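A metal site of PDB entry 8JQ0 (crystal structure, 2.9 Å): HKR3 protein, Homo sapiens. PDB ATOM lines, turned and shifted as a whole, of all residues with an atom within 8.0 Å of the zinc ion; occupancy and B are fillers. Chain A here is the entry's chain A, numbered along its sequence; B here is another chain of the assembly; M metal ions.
ND1 of His 21 is in hydrogen-bond range of OP2 of DG 12 of chain B (3.0 Å). A ring nitrogen (ND1) of His 25 sits at hydrogen-bond distance from the side-chain amide nitrogen (ND2) of Asn 68 (3.1 Å). ND1 of His 25 is in hydrogen-bond range of O of Leu 69 (3.0 Å). The side-chain sulfur (SG) of Cys 5 sits close to the backbone NH (N) of Ile 7, 3.3 Å away.
Ile 7 touches the zinc ion. Five residues have an atom within 4 Å of the zinc ion: Cys 5, Ile 7, Cys 8, His 21 and His 25. The nearest printed residue that does not touch the zinc ion is Gly 9 (5.1 Å).
The zinc ion is bound by NE2 of His 21 (2.1 Å). NE2 of His 25 binds the zinc ion (2.3 Å). SG of Cys 8 is bound to the zinc ion (2.3 Å). The zinc ion is bound by SG of Cys 5, 2.6 Å away.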
ATOM      1  N   PHE A   4     -25.205  12.196  -6.307  1.00  0.00           N
ATOM      2  CA  PHE A   4     -24.549  11.054  -6.923  1.00  0.00           C
ATOM      3  C   PHE A   4     -23.079  11.373  -7.186  1.00  0.00           C
ATOM      4  O   PHE A   4     -22.626  12.504  -6.999  1.00  0.00           O
ATOM      5  CB  PHE A   4     -25.255  10.634  -8.216  1.00  0.00           C
ATOM      6  CG  PHE A   4     -25.125  11.629  -9.337  1.00  0.00           C
ATOM      7  CD1 PHE A   4     -25.819  12.830  -9.300  1.00  0.00           C
ATOM      8  CD2 PHE A   4     -24.318  11.361 -10.434  1.00  0.00           C
ATOM      9  CE1 PHE A   4     -25.704  13.742 -10.324  1.00  0.00           C
ATOM     10  CE2 PHE A   4     -24.203  12.273 -11.458  1.00  0.00           C
ATOM     11  CZ  PHE A   4     -24.897  13.472 -11.411  1.00  0.00           C
ATOM     12  N   CYS A   5     -22.349  10.358  -7.628  1.00  0.00           N
ATOM     13  CA  CYS A   5     -20.922  10.468  -7.886  1.00  0.00           C
ATOM     14  C   CYS A   5     -20.635  10.269  -9.361  1.00  0.00           C
ATOM     15  O   CYS A   5     -21.238   9.399 -10.006  1.00  0.00           O
ATOM     16  CB  CYS A   5     -20.146   9.437  -7.052  1.00  0.00           C
ATOM     17  SG  CYS A   5     -18.376   9.380  -7.400  1.00  0.00           S
ATOM     18  N   GLN A   6     -19.713  11.065  -9.906  1.00  0.00           N
ATOM     19  CA  GLN A   6     -19.377  10.959 -11.323  1.00  0.00           C
ATOM     20  C   GLN A   6     -18.550   9.722 -11.646  1.00  0.00           C
ATOM     21  O   GLN A   6     -18.311   9.453 -12.819  1.00  0.00           O
ATOM     22  CB  GLN A   6     -18.623  12.209 -11.788  1.00  0.00           C
ATOM     23  CG  GLN A   6     -19.375  13.511 -11.574  1.00  0.00           C
ATOM     24  CD  GLN A   6     -19.119  14.106 -10.213  1.00  0.00           C
ATOM     25  OE1 GLN A   6     -19.474  13.527  -9.192  1.00  0.00           O
ATOM     26  NE2 GLN A   6     -18.491  15.275 -10.197  1.00  0.00           N
ATOM     27  N   ILE A   7     -18.109   8.974 -10.632  1.00  0.00           N
ATOM     28  CA  ILE A   7     -17.346   7.758 -10.872  1.00  0.00           C
ATOM     29  C   ILE A   7     -18.256   6.537 -10.965  1.00  0.00           C
ATOM     30  O   ILE A   7     -18.210   5.796 -11.946  1.00  0.00           O
ATOM     31  CB  ILE A   7     -16.283   7.588  -9.767  1.00  0.00           C
ATOM     32  CG1 ILE A   7     -15.560   8.906  -9.502  1.00  0.00           C
ATOM     33  CG2 ILE A   7     -15.282   6.510 -10.151  1.00  0.00           C
ATOM     34  CD1 ILE A   7     -14.650   9.337 -10.624  1.00  0.00           C
ATOM     35  N   CYS A   8     -19.104   6.322  -9.958  1.00  0.00           N
ATOM     36  CA  CYS A   8     -20.009   5.179  -9.946  1.00  0.00           C
ATOM     37  C   CYS A   8     -21.416   5.524 -10.382  1.00  0.00           C
ATOM     38  O   CYS A   8     -22.082   4.683 -10.994  1.00  0.00           O
ATOM     39  CB  CYS A   8     -20.070   4.563  -8.548  1.00  0.00           C
ATOM     40  SG  CYS A   8     -18.653   4.895  -7.494  1.00  0.00           S
ATOM     41  N   GLY A   9     -21.886   6.722 -10.077  1.00  0.00           N
ATOM     42  CA  GLY A   9     -23.299   7.032 -10.164  1.00  0.00           C
ATOM     43  C   GLY A   9     -24.079   6.660  -8.928  1.00  0.00           C
ATOM     44  O   GLY A   9     -25.293   6.886  -8.893  1.00  0.00           O
ATOM     45  N   LYS A  10     -23.419   6.091  -7.920  1.00  0.00           N
ATOM     46  CA  LYS A  10     -24.088   5.686  -6.696  1.00  0.00           C
ATOM     47  C   LYS A  10     -24.639   6.906  -5.963  1.00  0.00           C
ATOM     48  O   LYS A  10     -23.886   7.835  -5.639  1.00  0.00           O
ATOM     49  CB  LYS A  10     -23.123   4.920  -5.803  1.00  0.00           C
ATOM     50  CG  LYS A  10     -23.744   3.747  -5.068  1.00  0.00           C
ATOM     51  CD  LYS A  10     -22.698   2.955  -4.299  1.00  0.00           C
ATOM     52  CE  LYS A  10     -23.090   2.794  -2.846  1.00  0.00           C
ATOM     53  NZ  LYS A  10     -24.347   2.019  -2.702  1.00  0.00           N
ATOM     54  N   THR A  11     -25.939   6.900  -5.694  1.00  0.00           N
ATOM     55  CA  THR A  11     -26.579   8.008  -5.022  1.00  0.00           C
ATOM     56  C   THR A  11     -26.330   7.950  -3.525  1.00  0.00           C
ATOM     57  O   THR A  11     -26.180   6.879  -2.936  1.00  0.00           O
ATOM     58  CB  THR A  11     -28.088   8.007  -5.295  1.00  0.00           C
ATOM     59  OG1 THR A  11     -28.559   6.650  -5.348  1.00  0.00           O
ATOM     60  CG2 THR A  11     -28.392   8.695  -6.620  1.00  0.00           C
ATOM     61  N   PHE A  12     -26.285   9.131  -2.904  1.00  0.00           N
ATOM     62  CA  PHE A  12     -26.079   9.242  -1.461  1.00  0.00           C
ATOM     63  C   PHE A  12     -27.046  10.275  -0.902  1.00  0.00           C
ATOM     64  O   PHE A  12     -27.160  11.373  -1.445  1.00  0.00           O
ATOM     65  CB  PHE A  12     -24.633   9.622  -1.128  1.00  0.00           C
ATOM     66  CG  PHE A  12     -23.648   8.504  -1.367  1.00  0.00           C
ATOM     67  CD1 PHE A  12     -23.325   7.629  -0.346  1.00  0.00           C
ATOM     68  CD2 PHE A  12     -23.049   8.342  -2.604  1.00  0.00           C
ATOM     69  CE1 PHE A  12     -22.427   6.608  -0.551  1.00  0.00           C
ATOM     70  CE2 PHE A  12     -22.144   7.316  -2.809  1.00  0.00           C
ATOM     71  CZ  PHE A  12     -21.836   6.453  -1.787  1.00  0.00           C
ATOM     72  N   LEU A  18     -21.457  11.085   0.878  1.00  0.00           N
ATOM     73  CA  LEU A  18     -20.990  10.999  -0.503  1.00  0.00           C
ATOM     74  C   LEU A  18     -19.527  11.406  -0.600  1.00  0.00           C
ATOM     75  O   LEU A  18     -18.752  10.778  -1.332  1.00  0.00           O
ATOM     76  CB  LEU A  18     -21.857  11.882  -1.404  1.00  0.00           C
ATOM     77  CG  LEU A  18     -21.199  12.430  -2.676  1.00  0.00           C
ATOM     78  CD1 LEU A  18     -21.022  11.336  -3.722  1.00  0.00           C
ATOM     79  CD2 LEU A  18     -21.981  13.606  -3.244  1.00  0.00           C
ATOM     80  N   HIS A  21     -17.188   8.850   0.320  1.00  0.00           N
ATOM     81  CA  HIS A  21     -17.154   7.793  -0.684  1.00  0.00           C
ATOM     82  C   HIS A  21     -16.217   8.144  -1.828  1.00  0.00           C
ATOM     83  O   HIS A  21     -15.517   7.268  -2.349  1.00  0.00           O
ATOM     84  CB  HIS A  21     -18.564   7.536  -1.209  1.00  0.00           C
ATOM     85  CG  HIS A  21     -18.597   6.869  -2.546  1.00  0.00           C
ATOM     86  ND1 HIS A  21     -18.405   5.513  -2.713  1.00  0.00           N
ATOM     87  CD2 HIS A  21     -18.799   7.364  -3.788  1.00  0.00           C
ATOM     88  CE1 HIS A  21     -18.477   5.207  -3.991  1.00  0.00           C
ATOM     89  NE2 HIS A  21     -18.721   6.314  -4.668  1.00  0.00           N
ATOM     90  N   VAL A  22     -16.171   9.424  -2.226  1.00  0.00           N
ATOM     91  CA  VAL A  22     -15.208   9.845  -3.236  1.00  0.00           C
ATOM     92  C   VAL A  22     -13.790   9.739  -2.699  1.00  0.00           C
ATOM     93  O   VAL A  22     -12.835   9.527  -3.469  1.00  0.00           O
ATOM     94  CB  VAL A  22     -15.527  11.266  -3.731  1.00  0.00           C
ATOM     95  CG1 VAL A  22     -14.894  11.505  -5.085  1.00  0.00           C
ATOM     96  CG2 VAL A  22     -17.020  11.482  -3.806  1.00  0.00           C
ATOM     97  N   ARG A  23     -13.604   9.890  -1.392  1.00  0.00           N
ATOM     98  CA  ARG A  23     -12.289   9.688  -0.803  1.00  0.00           C
ATOM     99  C   ARG A  23     -11.851   8.232  -0.888  1.00  0.00           C
ATOM    100  O   ARG A  23     -10.658   7.941  -0.895  1.00  0.00           O
ATOM    101  CB  ARG A  23     -12.271  10.167   0.654  1.00  0.00           C
ATOM    102  CG  ARG A  23     -12.476  11.658   0.823  1.00  0.00           C
ATOM    103  CD  ARG A  23     -12.904  12.012   2.238  1.00  0.00           C
ATOM    104  NE  ARG A  23     -11.823  11.816   3.207  1.00  0.00           N
ATOM    105  CZ  ARG A  23     -11.976  11.269   4.401  1.00  0.00           C
ATOM    106  NH1 ARG A  23     -13.154  10.851   4.829  1.00  0.00           N
ATOM    107  NH2 ARG A  23     -10.919  11.147   5.199  1.00  0.00           N
ATOM    108  N   ARG A  24     -12.811   7.309  -0.943  1.00  0.00           N
ATOM    109  CA  ARG A  24     -12.489   5.892  -1.106  1.00  0.00           C
ATOM    110  C   ARG A  24     -12.013   5.552  -2.518  1.00  0.00           C
ATOM    111  O   ARG A  24     -11.492   4.461  -2.724  1.00  0.00           O
ATOM    112  CB  ARG A  24     -13.700   5.032  -0.752  1.00  0.00           C
ATOM    113  CG  ARG A  24     -13.912   4.841   0.742  1.00  0.00           C
ATOM    114  CD  ARG A  24     -15.360   4.510   1.055  1.00  0.00           C
ATOM    115  NE  ARG A  24     -15.626   4.472   2.491  1.00  0.00           N
ATOM    116  CZ  ARG A  24     -16.744   4.895   3.058  1.00  0.00           C
ATOM    117  NH1 ARG A  24     -17.737   5.399   2.334  1.00  0.00           N
ATOM    118  NH2 ARG A  24     -16.882   4.808   4.379  1.00  0.00           N
ATOM    119  N   HIS A  25     -12.174   6.470  -3.477  1.00  0.00           N
ATOM    120  CA  HIS A  25     -11.782   6.198  -4.849  1.00  0.00           C
ATOM    121  C   HIS A  25     -10.280   6.318  -5.054  1.00  0.00           C
ATOM    122  O   HIS A  25      -9.715   5.584  -5.869  1.00  0.00           O
ATOM    123  CB  HIS A  25     -12.511   7.141  -5.808  1.00  0.00           C
ATOM    124  CG  HIS A  25     -13.878   6.671  -6.185  1.00  0.00           C
ATOM    125  ND1 HIS A  25     -14.126   5.398  -6.643  1.00  0.00           N
ATOM    126  CD2 HIS A  25     -15.076   7.310  -6.183  1.00  0.00           C
ATOM    127  CE1 HIS A  25     -15.409   5.262  -6.902  1.00  0.00           C
ATOM    128  NE2 HIS A  25     -16.013   6.402  -6.630  1.00  0.00           N
ATOM    129  N   ASN A  68     -14.469  -0.254  -5.977  1.00  0.00           N
ATOM    130  CA  ASN A  68     -14.705   0.904  -6.828  1.00  0.00           C
ATOM    131  C   ASN A  68     -13.386   1.499  -7.283  1.00  0.00           C
ATOM    132  O   ASN A  68     -12.401   1.506  -6.547  1.00  0.00           O
ATOM    133  CB  ASN A  68     -15.528   1.972  -6.086  1.00  0.00           C
ATOM    134  CG  ASN A  68     -15.066   2.198  -4.669  1.00  0.00           C
ATOM    135  OD1 ASN A  68     -15.518   1.533  -3.735  1.00  0.00           O
ATOM    136  ND2 ASN A  68     -14.150   3.146  -4.489  1.00  0.00           N
ATOM    137  N   LEU A  69     -13.363   1.977  -8.532  1.00  0.00           N
ATOM    138  CA  LEU A  69     -12.156   2.541  -9.118  1.00  0.00           C
ATOM    139  C   LEU A  69     -11.858   3.939  -8.577  1.00  0.00           C
ATOM    140  O   LEU A  69     -11.531   4.096  -7.397  1.00  0.00           O
ATOM    141  CB  LEU A  69     -12.274   2.593 -10.643  1.00  0.00           C
ATOM    142  CG  LEU A  69     -13.197   3.663 -11.222  1.00  0.00           C
ATOM    143  CD1 LEU A  69     -12.617   4.258 -12.498  1.00  0.00           C
ATOM    144  CD2 LEU A  69     -14.585   3.098 -11.472  1.00  0.00           C
ATOM    145  P    DG B  12     -19.059   2.663  -0.572  1.00  0.00           P
ATOM    146  OP1  DG B  12     -19.874   2.543  -1.809  1.00  0.00           O
ATOM    147  OP2  DG B  12     -17.840   3.507  -0.594  1.00  0.00           O
ATOM    148  O5'  DG B  12     -20.014   3.142   0.607  1.00  0.00           O
ATOM    149  C5'  DG B  12     -21.404   3.300   0.363  1.00  0.00           C
ATOM    150  C4'  DG B  12     -22.230   2.680   1.477  1.00  0.00           C
ATOM    151  O4'  DG B  12     -21.564   1.519   2.023  1.00  0.00           O
ATOM    152  C3'  DG B  12     -22.450   3.560   2.690  1.00  0.00           C
ATOM    153  O3'  DG B  12     -23.465   4.514   2.434  1.00  0.00           O
ATOM    154  C2'  DG B  12     -22.877   2.527   3.726  1.00  0.00           C
ATOM    155  C1'  DG B  12     -21.983   1.335   3.371  1.00  0.00           C
ATOM    156  N9   DG B  12     -20.803   1.236   4.227  1.00  0.00           N
ATOM    157  C8   DG B  12     -19.523   1.641   3.932  1.00  0.00           C
ATOM    158  N7   DG B  12     -18.677   1.429   4.913  1.00  0.00           N
ATOM    159  C5   DG B  12     -19.453   0.857   5.914  1.00  0.00           C
ATOM    160  C6   DG B  12     -19.083   0.415   7.209  1.00  0.00           C
ATOM    161  O6   DG B  12     -17.969   0.438   7.739  1.00  0.00           O
ATOM    162  N1   DG B  12     -20.182  -0.099   7.907  1.00  0.00           N
ATOM    163  C2   DG B  12     -21.461  -0.182   7.414  1.00  0.00           C
ATOM    164  N2   DG B  12     -22.385  -0.711   8.225  1.00  0.00           N
ATOM    165  N3   DG B  12     -21.817   0.234   6.196  1.00  0.00           N
ATOM    166  C4   DG B  12     -20.767   0.733   5.504  1.00  0.00           C
HETATM  167 ZN    ZN M   1     -18.195   6.955  -6.596  1.00  0.00          ZN
